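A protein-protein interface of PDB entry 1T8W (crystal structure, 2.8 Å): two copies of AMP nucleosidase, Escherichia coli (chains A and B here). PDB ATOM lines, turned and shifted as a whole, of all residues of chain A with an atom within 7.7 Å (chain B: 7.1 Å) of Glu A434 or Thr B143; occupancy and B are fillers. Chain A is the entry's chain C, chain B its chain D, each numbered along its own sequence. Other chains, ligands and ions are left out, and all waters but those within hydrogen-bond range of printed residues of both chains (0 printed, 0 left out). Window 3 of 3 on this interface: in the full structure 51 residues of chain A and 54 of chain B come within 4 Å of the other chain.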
ATOM      1  N   GLY A 307     -10.171   1.155  -9.999  1.00  0.00           N
ATOM      2  CA  GLY A 307     -10.944   2.250  -9.462  1.00  0.00           C
ATOM      3  C   GLY A 307     -11.030   2.060  -7.956  1.00  0.00           C
ATOM      4  O   GLY A 307     -11.178   0.942  -7.466  1.00  0.00           O
ATOM      5  N   GLY A 308     -10.907   3.154  -7.220  1.00  0.00           N
ATOM      6  CA  GLY A 308     -11.002   3.101  -5.778  1.00  0.00           C
ATOM      7  C   GLY A 308     -12.460   3.318  -5.442  1.00  0.00           C
ATOM      8  O   GLY A 308     -13.064   4.310  -5.873  1.00  0.00           O
ATOM      9  N   GLN A 313      -9.863   6.412   0.140  1.00  0.00           N
ATOM     10  CA  GLN A 313      -8.789   6.117  -0.813  1.00  0.00           C
ATOM     11  C   GLN A 313      -8.400   7.333  -1.634  1.00  0.00           C
ATOM     12  O   GLN A 313      -9.234   8.166  -1.952  1.00  0.00           O
ATOM     13  CB  GLN A 313      -9.206   5.009  -1.773  1.00  0.00           C
ATOM     14  CG  GLN A 313      -9.003   3.623  -1.263  1.00  0.00           C
ATOM     15  CD  GLN A 313      -9.615   2.594  -2.166  1.00  0.00           C
ATOM     16  OE1 GLN A 313      -9.097   1.496  -2.289  1.00  0.00           O
ATOM     17  NE2 GLN A 313     -10.727   2.935  -2.798  1.00  0.00           N
ATOM     18  N   ALA A 314      -7.127   7.415  -1.986  1.00  0.00           N
ATOM     19  CA  ALA A 314      -6.607   8.522  -2.773  1.00  0.00           C
ATOM     20  C   ALA A 314      -5.965   7.984  -4.035  1.00  0.00           C
ATOM     21  O   ALA A 314      -5.329   6.928  -4.011  1.00  0.00           O
ATOM     22  CB  ALA A 314      -5.584   9.284  -1.982  1.00  0.00           C
ATOM     23  N   ILE A 315      -6.138   8.702  -5.140  1.00  0.00           N
ATOM     24  CA  ILE A 315      -5.541   8.275  -6.393  1.00  0.00           C
ATOM     25  C   ILE A 315      -4.049   8.073  -6.152  1.00  0.00           C
ATOM     26  O   ILE A 315      -3.387   8.950  -5.608  1.00  0.00           O
ATOM     27  CB  ILE A 315      -5.751   9.320  -7.502  1.00  0.00           C
ATOM     28  CG1 ILE A 315      -7.218   9.320  -7.936  1.00  0.00           C
ATOM     29  CG2 ILE A 315      -4.844   9.020  -8.665  1.00  0.00           C
ATOM     30  CD1 ILE A 315      -7.530  10.241  -9.080  1.00  0.00           C
ATOM     31  N   SER A 427      -6.342   4.379  -9.874  1.00  0.00           N
ATOM     32  CA  SER A 427      -6.131   5.389 -10.908  1.00  0.00           C
ATOM     33  C   SER A 427      -7.256   6.433 -10.894  1.00  0.00           C
ATOM     34  O   SER A 427      -7.188   7.464 -11.557  1.00  0.00           O
ATOM     35  CB  SER A 427      -5.993   4.740 -12.293  1.00  0.00           C
ATOM     36  OG  SER A 427      -7.220   4.263 -12.789  1.00  0.00           O
ATOM     37  N   ASP A 428      -8.294   6.176 -10.113  1.00  0.00           N
ATOM     38  CA  ASP A 428      -9.392   7.126 -10.017  1.00  0.00           C
ATOM     39  C   ASP A 428     -10.439   6.658  -9.030  1.00  0.00           C
ATOM     40  O   ASP A 428     -10.370   5.548  -8.537  1.00  0.00           O
ATOM     41  CB  ASP A 428     -10.027   7.359 -11.389  1.00  0.00           C
ATOM     42  CG  ASP A 428     -10.801   6.171 -11.879  1.00  0.00           C
ATOM     43  OD1 ASP A 428     -10.206   5.078 -12.001  1.00  0.00           O
ATOM     44  OD2 ASP A 428     -12.007   6.331 -12.150  1.00  0.00           O
ATOM     45  N   LYS A 429     -11.402   7.519  -8.744  1.00  0.00           N
ATOM     46  CA  LYS A 429     -12.452   7.201  -7.801  1.00  0.00           C
ATOM     47  C   LYS A 429     -13.792   7.504  -8.435  1.00  0.00           C
ATOM     48  O   LYS A 429     -14.321   8.599  -8.287  1.00  0.00           O
ATOM     49  CB  LYS A 429     -12.234   8.012  -6.538  1.00  0.00           C
ATOM     50  CG  LYS A 429     -10.863   7.757  -5.954  1.00  0.00           C
ATOM     51  CD  LYS A 429     -10.678   8.463  -4.642  1.00  0.00           C
ATOM     52  CE  LYS A 429     -11.570   7.892  -3.572  1.00  0.00           C
ATOM     53  NZ  LYS A 429     -11.318   6.447  -3.545  1.00  0.00           N
ATOM     54  N   PRO A 430     -14.364   6.513  -9.139  1.00  0.00           N
ATOM     55  CA  PRO A 430     -15.638   6.517  -9.866  1.00  0.00           C
ATOM     56  C   PRO A 430     -16.833   6.985  -9.058  1.00  0.00           C
ATOM     57  O   PRO A 430     -17.727   7.647  -9.574  1.00  0.00           O
ATOM     58  CB  PRO A 430     -15.807   5.061 -10.276  1.00  0.00           C
ATOM     59  CG  PRO A 430     -14.445   4.506 -10.204  1.00  0.00           C
ATOM     60  CD  PRO A 430     -13.878   5.133  -8.999  1.00  0.00           C
ATOM     61  N   LEU A 431     -16.841   6.607  -7.785  1.00  0.00           N
ATOM     62  CA  LEU A 431     -17.920   6.936  -6.878  1.00  0.00           C
ATOM     63  C   LEU A 431     -17.758   8.275  -6.169  1.00  0.00           C
ATOM     64  O   LEU A 431     -18.629   8.681  -5.421  1.00  0.00           O
ATOM     65  CB  LEU A 431     -18.043   5.822  -5.845  1.00  0.00           C
ATOM     66  CG  LEU A 431     -18.907   4.601  -6.170  1.00  0.00           C
ATOM     67  CD1 LEU A 431     -18.979   4.292  -7.654  1.00  0.00           C
ATOM     68  CD2 LEU A 431     -18.334   3.450  -5.376  1.00  0.00           C
ATOM     69  N   HIS A 432     -16.646   8.962  -6.402  1.00  0.00           N
ATOM     70  CA  HIS A 432     -16.415  10.231  -5.738  1.00  0.00           C
ATOM     71  C   HIS A 432     -15.969  11.368  -6.635  1.00  0.00           C
ATOM     72  O   HIS A 432     -14.978  12.033  -6.352  1.00  0.00           O
ATOM     73  CB  HIS A 432     -15.413  10.051  -4.606  1.00  0.00           C
ATOM     74  CG  HIS A 432     -15.776   8.954  -3.660  1.00  0.00           C
ATOM     75  ND1 HIS A 432     -15.761   7.625  -4.023  1.00  0.00           N
ATOM     76  CD2 HIS A 432     -16.191   8.988  -2.374  1.00  0.00           C
ATOM     77  CE1 HIS A 432     -16.153   6.887  -3.001  1.00  0.00           C
ATOM     78  NE2 HIS A 432     -16.420   7.690  -1.988  1.00  0.00           N
ATOM     79  N   GLY A 433     -16.686  11.580  -7.731  1.00  0.00           N
ATOM     80  CA  GLY A 433     -16.375  12.698  -8.605  1.00  0.00           C
ATOM     81  C   GLY A 433     -15.134  12.726  -9.466  1.00  0.00           C
ATOM     82  O   GLY A 433     -14.971  13.664 -10.247  1.00  0.00           O
ATOM     83  N   GLU A 434     -14.265  11.729  -9.345  1.00  0.00           N
ATOM     84  CA  GLU A 434     -13.059  11.687 -10.163  1.00  0.00           C
ATOM     85  C   GLU A 434     -12.980  10.506 -11.128  1.00  0.00           C
ATOM     86  O   GLU A 434     -12.169   9.609 -10.944  1.00  0.00           O
ATOM     87  CB  GLU A 434     -11.819  11.703  -9.273  1.00  0.00           C
ATOM     88  CG  GLU A 434     -11.395  13.097  -8.887  1.00  0.00           C
ATOM     89  CD  GLU A 434     -10.002  13.152  -8.277  1.00  0.00           C
ATOM     90  OE1 GLU A 434      -9.761  12.371  -7.319  1.00  0.00           O
ATOM     91  OE2 GLU A 434      -9.163  13.975  -8.751  1.00  0.00           O
ATOM     92  N   ILE A 435     -13.805  10.505 -12.167  1.00  0.00           N
ATOM     93  CA  ILE A 435     -13.764   9.398 -13.120  1.00  0.00           C
ATOM     94  C   ILE A 435     -12.709   9.606 -14.217  1.00  0.00           C
ATOM     95  O   ILE A 435     -13.060   9.846 -15.377  1.00  0.00           O
ATOM     96  CB  ILE A 435     -15.131   9.166 -13.838  1.00  0.00           C
ATOM     97  CG1 ILE A 435     -16.301   9.463 -12.907  1.00  0.00           C
ATOM     98  CG2 ILE A 435     -15.228   7.705 -14.298  1.00  0.00           C
ATOM     99  CD1 ILE A 435     -17.658   9.080 -13.508  1.00  0.00           C
ATOM    100  N   LYS A 436     -11.428   9.504 -13.860  1.00  0.00           N
ATOM    101  CA  LYS A 436     -10.327   9.664 -14.819  1.00  0.00           C
ATOM    102  C   LYS A 436     -10.069   8.398 -15.663  1.00  0.00           C
ATOM    103  O   LYS A 436     -10.256   7.276 -15.185  1.00  0.00           O
ATOM    104  CB  LYS A 436      -9.062  10.055 -14.062  1.00  0.00           C
ATOM    105  CG  LYS A 436      -9.248  11.304 -13.231  1.00  0.00           C
ATOM    106  CD  LYS A 436      -7.968  11.734 -12.524  1.00  0.00           C
ATOM    107  CE  LYS A 436      -7.944  13.245 -12.382  1.00  0.00           C
ATOM    108  NZ  LYS A 436      -8.064  13.896 -13.741  1.00  0.00           N
ATOM    109  N   LEU A 437      -9.648   8.578 -16.914  1.00  0.00           N
ATOM    110  CA  LEU A 437      -9.365   7.448 -17.811  1.00  0.00           C
ATOM    111  C   LEU A 437      -7.874   7.236 -18.081  1.00  0.00           C
ATOM    112  O   LEU A 437      -7.086   8.191 -18.090  1.00  0.00           O
ATOM    113  CB  LEU A 437     -10.063   7.634 -19.154  1.00  0.00           C
ATOM    114  CG  LEU A 437     -11.553   7.325 -19.230  1.00  0.00           C
ATOM    115  CD1 LEU A 437     -12.317   8.020 -18.111  1.00  0.00           C
ATOM    116  CD2 LEU A 437     -12.055   7.778 -20.583  1.00  0.00           C
ATOM    117  N   GLN A 440      -5.758   9.853 -20.076  1.00  0.00           N
ATOM    118  CA  GLN A 440      -6.078  11.216 -19.686  1.00  0.00           C
ATOM    119  C   GLN A 440      -4.976  11.670 -18.731  1.00  0.00           C
ATOM    120  O   GLN A 440      -4.182  10.856 -18.245  1.00  0.00           O
ATOM    121  CB  GLN A 440      -7.402  11.283 -18.916  1.00  0.00           C
ATOM    122  CG  GLN A 440      -8.689  11.147 -19.715  1.00  0.00           C
ATOM    123  CD  GLN A 440      -9.922  11.357 -18.820  1.00  0.00           C
ATOM    124  OE1 GLN A 440     -11.076  11.209 -19.263  1.00  0.00           O
ATOM    125  NE2 GLN A 440      -9.678  11.708 -17.550  1.00  0.00           N
ATOM    126  N   ASN A 442      -3.372  12.514 -15.384  1.00  0.00           N
ATOM    127  CA  ASN A 442      -3.622  11.997 -14.065  1.00  0.00           C
ATOM    128  C   ASN A 442      -2.352  12.212 -13.275  1.00  0.00           C
ATOM    129  O   ASN A 442      -1.596  11.286 -13.002  1.00  0.00           O
ATOM    130  CB  ASN A 442      -3.954  10.521 -14.146  1.00  0.00           C
ATOM    131  CG  ASN A 442      -4.779  10.072 -12.993  1.00  0.00           C
ATOM    132  OD1 ASN A 442      -4.557  10.485 -11.858  1.00  0.00           O
ATOM    133  ND2 ASN A 442      -5.746   9.222 -13.268  1.00  0.00           N
ATOM    134  N   PHE A 444      -1.404  12.347 -10.310  1.00  0.00           N
ATOM    135  CA  PHE A 444      -1.056  11.401  -9.266  1.00  0.00           C
ATOM    136  C   PHE A 444      -1.003   9.909  -9.522  1.00  0.00           C
ATOM    137  O   PHE A 444      -0.388   9.180  -8.743  1.00  0.00           O
ATOM    138  CB  PHE A 444      -1.886  11.744  -8.042  1.00  0.00           C
ATOM    139  CG  PHE A 444      -1.563  13.104  -7.513  1.00  0.00           C
ATOM    140  CD1 PHE A 444      -2.451  14.165  -7.671  1.00  0.00           C
ATOM    141  CD2 PHE A 444      -0.312  13.353  -6.939  1.00  0.00           C
ATOM    142  CE1 PHE A 444      -2.094  15.460  -7.267  1.00  0.00           C
ATOM    143  CE2 PHE A 444       0.057  14.638  -6.532  1.00  0.00           C
ATOM    144  CZ  PHE A 444      -0.834  15.696  -6.696  1.00  0.00           C
ATOM    145  N   TYR B  35     -11.349  30.018  -8.793  1.00  0.00           N
ATOM    146  CA  TYR B  35     -10.959  29.145  -7.689  1.00  0.00           C
ATOM    147  C   TYR B  35      -9.479  28.787  -7.778  1.00  0.00           C
ATOM    148  O   TYR B  35      -8.802  28.643  -6.760  1.00  0.00           O
ATOM    149  CB  TYR B  35     -11.782  27.854  -7.684  1.00  0.00           C
ATOM    150  CG  TYR B  35     -11.380  26.921  -6.576  1.00  0.00           C
ATOM    151  CD1 TYR B  35     -11.767  27.168  -5.264  1.00  0.00           C
ATOM    152  CD2 TYR B  35     -10.527  25.847  -6.819  1.00  0.00           C
ATOM    153  CE1 TYR B  35     -11.308  26.379  -4.217  1.00  0.00           C
ATOM    154  CE2 TYR B  35     -10.059  25.052  -5.785  1.00  0.00           C
ATOM    155  CZ  TYR B  35     -10.449  25.327  -4.481  1.00  0.00           C
ATOM    156  OH  TYR B  35      -9.948  24.583  -3.434  1.00  0.00           O
ATOM    157  N   TYR B 123     -17.902  19.845 -14.008  1.00  0.00           N
ATOM    158  CA  TYR B 123     -16.760  20.644 -14.449  1.00  0.00           C
ATOM    159  C   TYR B 123     -15.829  20.005 -15.472  1.00  0.00           C
ATOM    160  O   TYR B 123     -15.332  20.687 -16.362  1.00  0.00           O
ATOM    161  CB  TYR B 123     -15.969  21.192 -13.235  1.00  0.00           C
ATOM    162  CG  TYR B 123     -14.978  20.261 -12.583  1.00  0.00           C
ATOM    163  CD1 TYR B 123     -13.719  20.036 -13.144  1.00  0.00           C
ATOM    164  CD2 TYR B 123     -15.309  19.581 -11.419  1.00  0.00           C
ATOM    165  CE1 TYR B 123     -12.821  19.148 -12.567  1.00  0.00           C
ATOM    166  CE2 TYR B 123     -14.421  18.690 -10.831  1.00  0.00           C
ATOM    167  CZ  TYR B 123     -13.177  18.473 -11.409  1.00  0.00           C
ATOM    168  OH  TYR B 123     -12.308  17.568 -10.829  1.00  0.00           O
ATOM    169  N   PRO B 124     -15.599  18.689 -15.384  1.00  0.00           N
ATOM    170  CA  PRO B 124     -14.712  18.056 -16.357  1.00  0.00           C
ATOM    171  C   PRO B 124     -15.130  18.268 -17.809  1.00  0.00           C
ATOM    172  O   PRO B 124     -14.291  18.316 -18.707  1.00  0.00           O
ATOM    173  CB  PRO B 124     -14.767  16.597 -15.954  1.00  0.00           C
ATOM    174  CG  PRO B 124     -14.924  16.685 -14.490  1.00  0.00           C
ATOM    175  CD  PRO B 124     -15.964  17.736 -14.327  1.00  0.00           C
ATOM    176  N   ARG B 136      -2.972  18.026  -4.816  1.00  0.00           N
ATOM    177  CA  ARG B 136      -3.948  17.346  -3.962  1.00  0.00           C
ATOM    178  C   ARG B 136      -5.088  18.237  -3.489  1.00  0.00           C
ATOM    179  O   ARG B 136      -6.247  17.997  -3.820  1.00  0.00           O
ATOM    180  CB  ARG B 136      -3.256  16.754  -2.738  1.00  0.00           C
ATOM    181  CG  ARG B 136      -2.243  15.671  -3.048  1.00  0.00           C
ATOM    182  CD  ARG B 136      -2.910  14.431  -3.591  1.00  0.00           C
ATOM    183  NE  ARG B 136      -1.945  13.370  -3.849  1.00  0.00           N
ATOM    184  CZ  ARG B 136      -2.256  12.197  -4.390  1.00  0.00           C
ATOM    185  NH1 ARG B 136      -3.510  11.927  -4.727  1.00  0.00           N
ATOM    186  NH2 ARG B 136      -1.306  11.303  -4.612  1.00  0.00           N
ATOM    187  N   SER B 137      -4.754  19.253  -2.699  1.00  0.00           N
ATOM    188  CA  SER B 137      -5.745  20.194  -2.169  1.00  0.00           C
ATOM    189  C   SER B 137      -6.581  20.848  -3.261  1.00  0.00           C
ATOM    190  O   SER B 137      -7.795  20.916  -3.164  1.00  0.00           O
ATOM    191  CB  SER B 137      -5.059  21.295  -1.363  1.00  0.00           C
ATOM    192  OG  SER B 137      -4.304  20.752  -0.303  1.00  0.00           O
ATOM    193  N   MET B 138      -5.921  21.348  -4.291  1.00  0.00           N
ATOM    194  CA  MET B 138      -6.613  21.985  -5.391  1.00  0.00           C
ATOM    195  C   MET B 138      -7.720  21.080  -5.915  1.00  0.00           C
ATOM    196  O   MET B 138      -8.860  21.506  -6.068  1.00  0.00           O
ATOM    197  CB  MET B 138      -5.626  22.285  -6.516  1.00  0.00           C
ATOM    198  CG  MET B 138      -4.646  23.418  -6.244  1.00  0.00           C
ATOM    199  SD  MET B 138      -5.499  25.150  -6.329  1.00  0.00           S
ATOM    200  CE  MET B 138      -5.375  25.512  -8.225  1.00  0.00           C
ATOM    201  N   SER B 139      -7.363  19.829  -6.189  1.00  0.00           N
ATOM    202  CA  SER B 139      -8.295  18.833  -6.712  1.00  0.00           C
ATOM    203  C   SER B 139      -9.428  18.576  -5.736  1.00  0.00           C
ATOM    204  O   SER B 139     -10.602  18.640  -6.099  1.00  0.00           O
ATOM    205  CB  SER B 139      -7.563  17.519  -6.985  1.00  0.00           C
ATOM    206  OG  SER B 139      -6.493  17.706  -7.890  1.00  0.00           O
ATOM    207  N   ALA B 140      -9.062  18.262  -4.500  1.00  0.00           N
ATOM    208  CA  ALA B 140     -10.038  18.004  -3.452  1.00  0.00           C
ATOM    209  C   ALA B 140     -11.040  19.143  -3.422  1.00  0.00           C
ATOM    210  O   ALA B 140     -12.241  18.927  -3.321  1.00  0.00           O
ATOM    211  CB  ALA B 140      -9.340  17.894  -2.112  1.00  0.00           C
ATOM    212  N   GLY B 141     -10.531  20.364  -3.518  1.00  0.00           N
ATOM    213  CA  GLY B 141     -11.387  21.528  -3.498  1.00  0.00           C
ATOM    214  C   GLY B 141     -12.306  21.572  -4.693  1.00  0.00           C
ATOM    215  O   GLY B 141     -13.459  21.961  -4.572  1.00  0.00           O
ATOM    216  N   LEU B 142     -11.796  21.182  -5.854  1.00  0.00           N
ATOM    217  CA  LEU B 142     -12.602  21.177  -7.068  1.00  0.00           C
ATOM    218  C   LEU B 142     -13.752  20.202  -6.941  1.00  0.00           C
ATOM    219  O   LEU B 142     -14.908  20.589  -7.045  1.00  0.00           O
ATOM    220  CB  LEU B 142     -11.768  20.798  -8.293  1.00  0.00           C
ATOM    221  CG  LEU B 142     -11.138  21.925  -9.100  1.00  0.00           C
ATOM    222  CD1 LEU B 142     -10.377  21.316 -10.246  1.00  0.00           C
ATOM    223  CD2 LEU B 142     -12.203  22.864  -9.626  1.00  0.00           C
ATOM    224  N   THR B 143     -13.440  18.934  -6.715  1.00  0.00           N
ATOM    225  CA  THR B 143     -14.491  17.931  -6.601  1.00  0.00           C
ATOM    226  C   THR B 143     -15.413  18.198  -5.417  1.00  0.00           C
ATOM    227  O   THR B 143     -16.521  17.665  -5.351  1.00  0.00           O
ATOM    228  CB  THR B 143     -13.913  16.477  -6.499  1.00  0.00           C
ATOM    229  OG1 THR B 143     -13.083  16.355  -5.339  1.00  0.00           O
ATOM    230  CG2 THR B 143     -13.100  16.135  -7.756  1.00  0.00           C
ATOM    231  N   ARG B 144     -14.974  19.050  -4.499  1.00  0.00           N
ATOM    232  CA  ARG B 144     -15.786  19.363  -3.334  1.00  0.00           C
ATOM    233  C   ARG B 144     -16.751  20.535  -3.510  1.00  0.00           C
ATOM    234  O   ARG B 144     -17.884  20.475  -3.048  1.00  0.00           O
ATOM    235  CB  ARG B 144     -14.898  19.638  -2.126  1.00  0.00           C
ATOM    236  CG  ARG B 144     -15.682  19.933  -0.865  1.00  0.00           C
ATOM    237  CD  ARG B 144     -14.767  20.233   0.312  1.00  0.00           C
ATOM    238  NE  ARG B 144     -15.533  20.478   1.533  1.00  0.00           N
ATOM    239  CZ  ARG B 144     -15.014  20.944   2.668  1.00  0.00           C
ATOM    240  NH1 ARG B 144     -13.716  21.218   2.747  1.00  0.00           N
ATOM    241  NH2 ARG B 144     -15.797  21.151   3.724  1.00  0.00           N
ATOM    242  N   TYR B 145     -16.312  21.597  -4.176  1.00  0.00           N
ATOM    243  CA  TYR B 145     -17.163  22.762  -4.354  1.00  0.00           C
ATOM    244  C   TYR B 145     -17.743  22.959  -5.747  1.00  0.00           C
ATOM    245  O   TYR B 145     -18.504  23.899  -5.974  1.00  0.00           O
ATOM    246  CB  TYR B 145     -16.395  24.022  -3.957  1.00  0.00           C
ATOM    247  CG  TYR B 145     -15.855  23.989  -2.553  1.00  0.00           C
ATOM    248  CD1 TYR B 145     -16.708  23.848  -1.458  1.00  0.00           C
ATOM    249  CD2 TYR B 145     -14.487  24.076  -2.313  1.00  0.00           C
ATOM    250  CE1 TYR B 145     -16.217  23.790  -0.159  1.00  0.00           C
ATOM    251  CE2 TYR B 145     -13.979  24.018  -1.014  1.00  0.00           C
ATOM    252  CZ  TYR B 145     -14.852  23.872   0.060  1.00  0.00           C
ATOM    253  OH  TYR B 145     -14.358  23.800   1.348  1.00  0.00           O
ATOM    254  N   PHE B 146     -17.397  22.086  -6.682  1.00  0.00           N
ATOM    255  CA  PHE B 146     -17.898  22.230  -8.038  1.00  0.00           C
ATOM    256  C   PHE B 146     -18.710  21.043  -8.518  1.00  0.00           C
ATOM    257  O   PHE B 146     -18.662  19.977  -7.926  1.00  0.00           O
ATOM    258  CB  PHE B 146     -16.730  22.478  -8.980  1.00  0.00           C
ATOM    259  CG  PHE B 146     -16.133  23.835  -8.837  1.00  0.00           C
ATOM    260  CD1 PHE B 146     -16.622  24.899  -9.577  1.00  0.00           C
ATOM    261  CD2 PHE B 146     -15.095  24.061  -7.941  1.00  0.00           C
ATOM    262  CE1 PHE B 146     -16.084  26.169  -9.425  1.00  0.00           C
ATOM    263  CE2 PHE B 146     -14.554  25.324  -7.784  1.00  0.00           C
ATOM    264  CZ  PHE B 146     -15.050  26.378  -8.526  1.00  0.00           C
ATOM    265  N   PRO B 147     -19.487  21.226  -9.593  1.00  0.00           N
ATOM    266  CA  PRO B 147     -20.317  20.161 -10.159  1.00  0.00           C
ATOM    267  C   PRO B 147     -19.466  18.971 -10.588  1.00  0.00           C
ATOM    268  O   PRO B 147     -18.572  19.112 -11.417  1.00  0.00           O
ATOM    269  CB  PRO B 147     -20.971  20.836 -11.363  1.00  0.00           C
ATOM    270  CG  PRO B 147     -21.023  22.255 -10.967  1.00  0.00           C
ATOM    271  CD  PRO B 147     -19.692  22.484 -10.328  1.00  0.00           C
ATOM    272  N   THR B 148     -19.737  17.801 -10.027  1.00  0.00           N
ATOM    273  CA  THR B 148     -18.993  16.606 -10.393  1.00  0.00           C
ATOM    274  C   THR B 148     -19.944  15.578 -10.973  1.00  0.00           C
ATOM    275  O   THR B 148     -21.152  15.728 -10.895  1.00  0.00           O
ATOM    276  CB  THR B 148     -18.278  15.985  -9.185  1.00  0.00           C
ATOM    277  OG1 THR B 148     -19.200  15.843  -8.101  1.00  0.00           O
ATOM    278  CG2 THR B 148     -17.134  16.854  -8.751  1.00  0.00           C
ATOM    279  N   THR B 149     -19.391  14.539 -11.574  1.00  0.00           N
ATOM    280  CA  THR B 149     -20.209  13.491 -12.152  1.00  0.00           C
ATOM    281  C   THR B 149     -20.635  12.554 -11.035  1.00  0.00           C
ATOM    282  O   THR B 149     -19.806  11.837 -10.480  1.00  0.00           O
ATOM    283  CB  THR B 149     -19.410  12.683 -13.180  1.00  0.00           C
ATOM    284  OG1 THR B 149     -18.026  13.053 -13.092  1.00  0.00           O
ATOM    285  CG2 THR B 149     -19.936  12.927 -14.592  1.00  0.00           C
ATOM    286  N   GLU B 150     -21.915  12.566 -10.687  1.00  0.00           N
ATOM    287  CA  GLU B 150     -22.405  11.674  -9.644  1.00  0.00           C
ATOM    288  C   GLU B 150     -23.144  10.542 -10.356  1.00  0.00           C
ATOM    289  O   GLU B 150     -23.837  10.775 -11.348  1.00  0.00           O
ATOM    290  CB  GLU B 150     -23.332  12.422  -8.669  1.00  0.00           C
ATOM    291  CG  GLU B 150     -22.654  13.598  -7.929  1.00  0.00           C
ATOM    292  CD  GLU B 150     -21.333  13.206  -7.235  1.00  0.00           C
ATOM    293  OE1 GLU B 150     -21.379  12.571  -6.148  1.00  0.00           O
ATOM    294  OE2 GLU B 150     -20.251  13.527  -7.789  1.00  0.00           O
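The backbone carbonyl oxygen of Ile A315 is in hydrogen-bond range of the guanidinium group of Arg B136, 3.1 Å away.
The side-chain carboxylate (OE2) of Glu B150 lies within hydrogen-bond range of the side-chain hydroxyl (OG1) of Thr B148. The backbone carbonyl oxygen of Glu A434 is in hydrogen-bond range of the backbone NH of Lys A429 (3.1 Å). The backbone carbonyl oxygen (O) of Ala B140 sits at hydrogen-bond distance from the side-chain hydroxyl (OG1) of Thr B143 (3.4 Å). The side-chain hydroxyl of Thr B143 sits at hydrogen-bond distance from the backbone carbonyl oxygen of Ser B139, 3.5 Å away.
CG2 of Thr B143 touches O of Gly A433, at 3.98 Å. Thr B148 touches Gly A433 (CB to CA, 3.8 Å). Glu A434 touches Thr B143. OG1 of Thr B149 touches CG1 of Ile A435, 3.99 Å away. Arg B136 touches Phe A444 (NH2 to CD2, 3.3 Å).
Printed residues of chain B within 4 Å of Gly A433: Thr B143 (3.98 Å) and Thr B148 (3.8 Å). Of the printed residues of chain B, Ile A435 touches Thr B149 (3.99 Å). Of the printed residues of chain B, Phe A444 touches Arg B136. Tyr B123 touches none of the printed residues of chain A. Of the printed residues of chain A, Arg B136 touches Ile A315 and Phe A444. Gly B141 touches none of the printed residues of chain A. Thr B143 touches two residues of chain A. Of the printed residues of chain A, Thr B148 touches Gly A433. The nearest residue of chain A that does not touch Thr B143 is His A432 (4.6 Å). The nearest printed residue of chain B that does not touch Ile A435 is Glu B150 (6.2 Å).
Of the 19 printed residues of chain A, 5 touch a printed residue of chain B. Hydrophobic or aromatic side chains of chain A that line the printed part of chain B: Ile A435 and Phe A444. Of the 18 printed residues of chain B, 4 touch a printed residue of chain A. Among the printed residues, 6 pairs touch across the chains. Among the printed residues, no Asp or Glu carboxylate lies within 4 Å of a Lys or Arg side-chain nitrogen of the other chain.
No position is printed for both chains. Of the 6 pairs that touch across the chains among the printed residues, none has its exchanged pair printed and touching as well.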
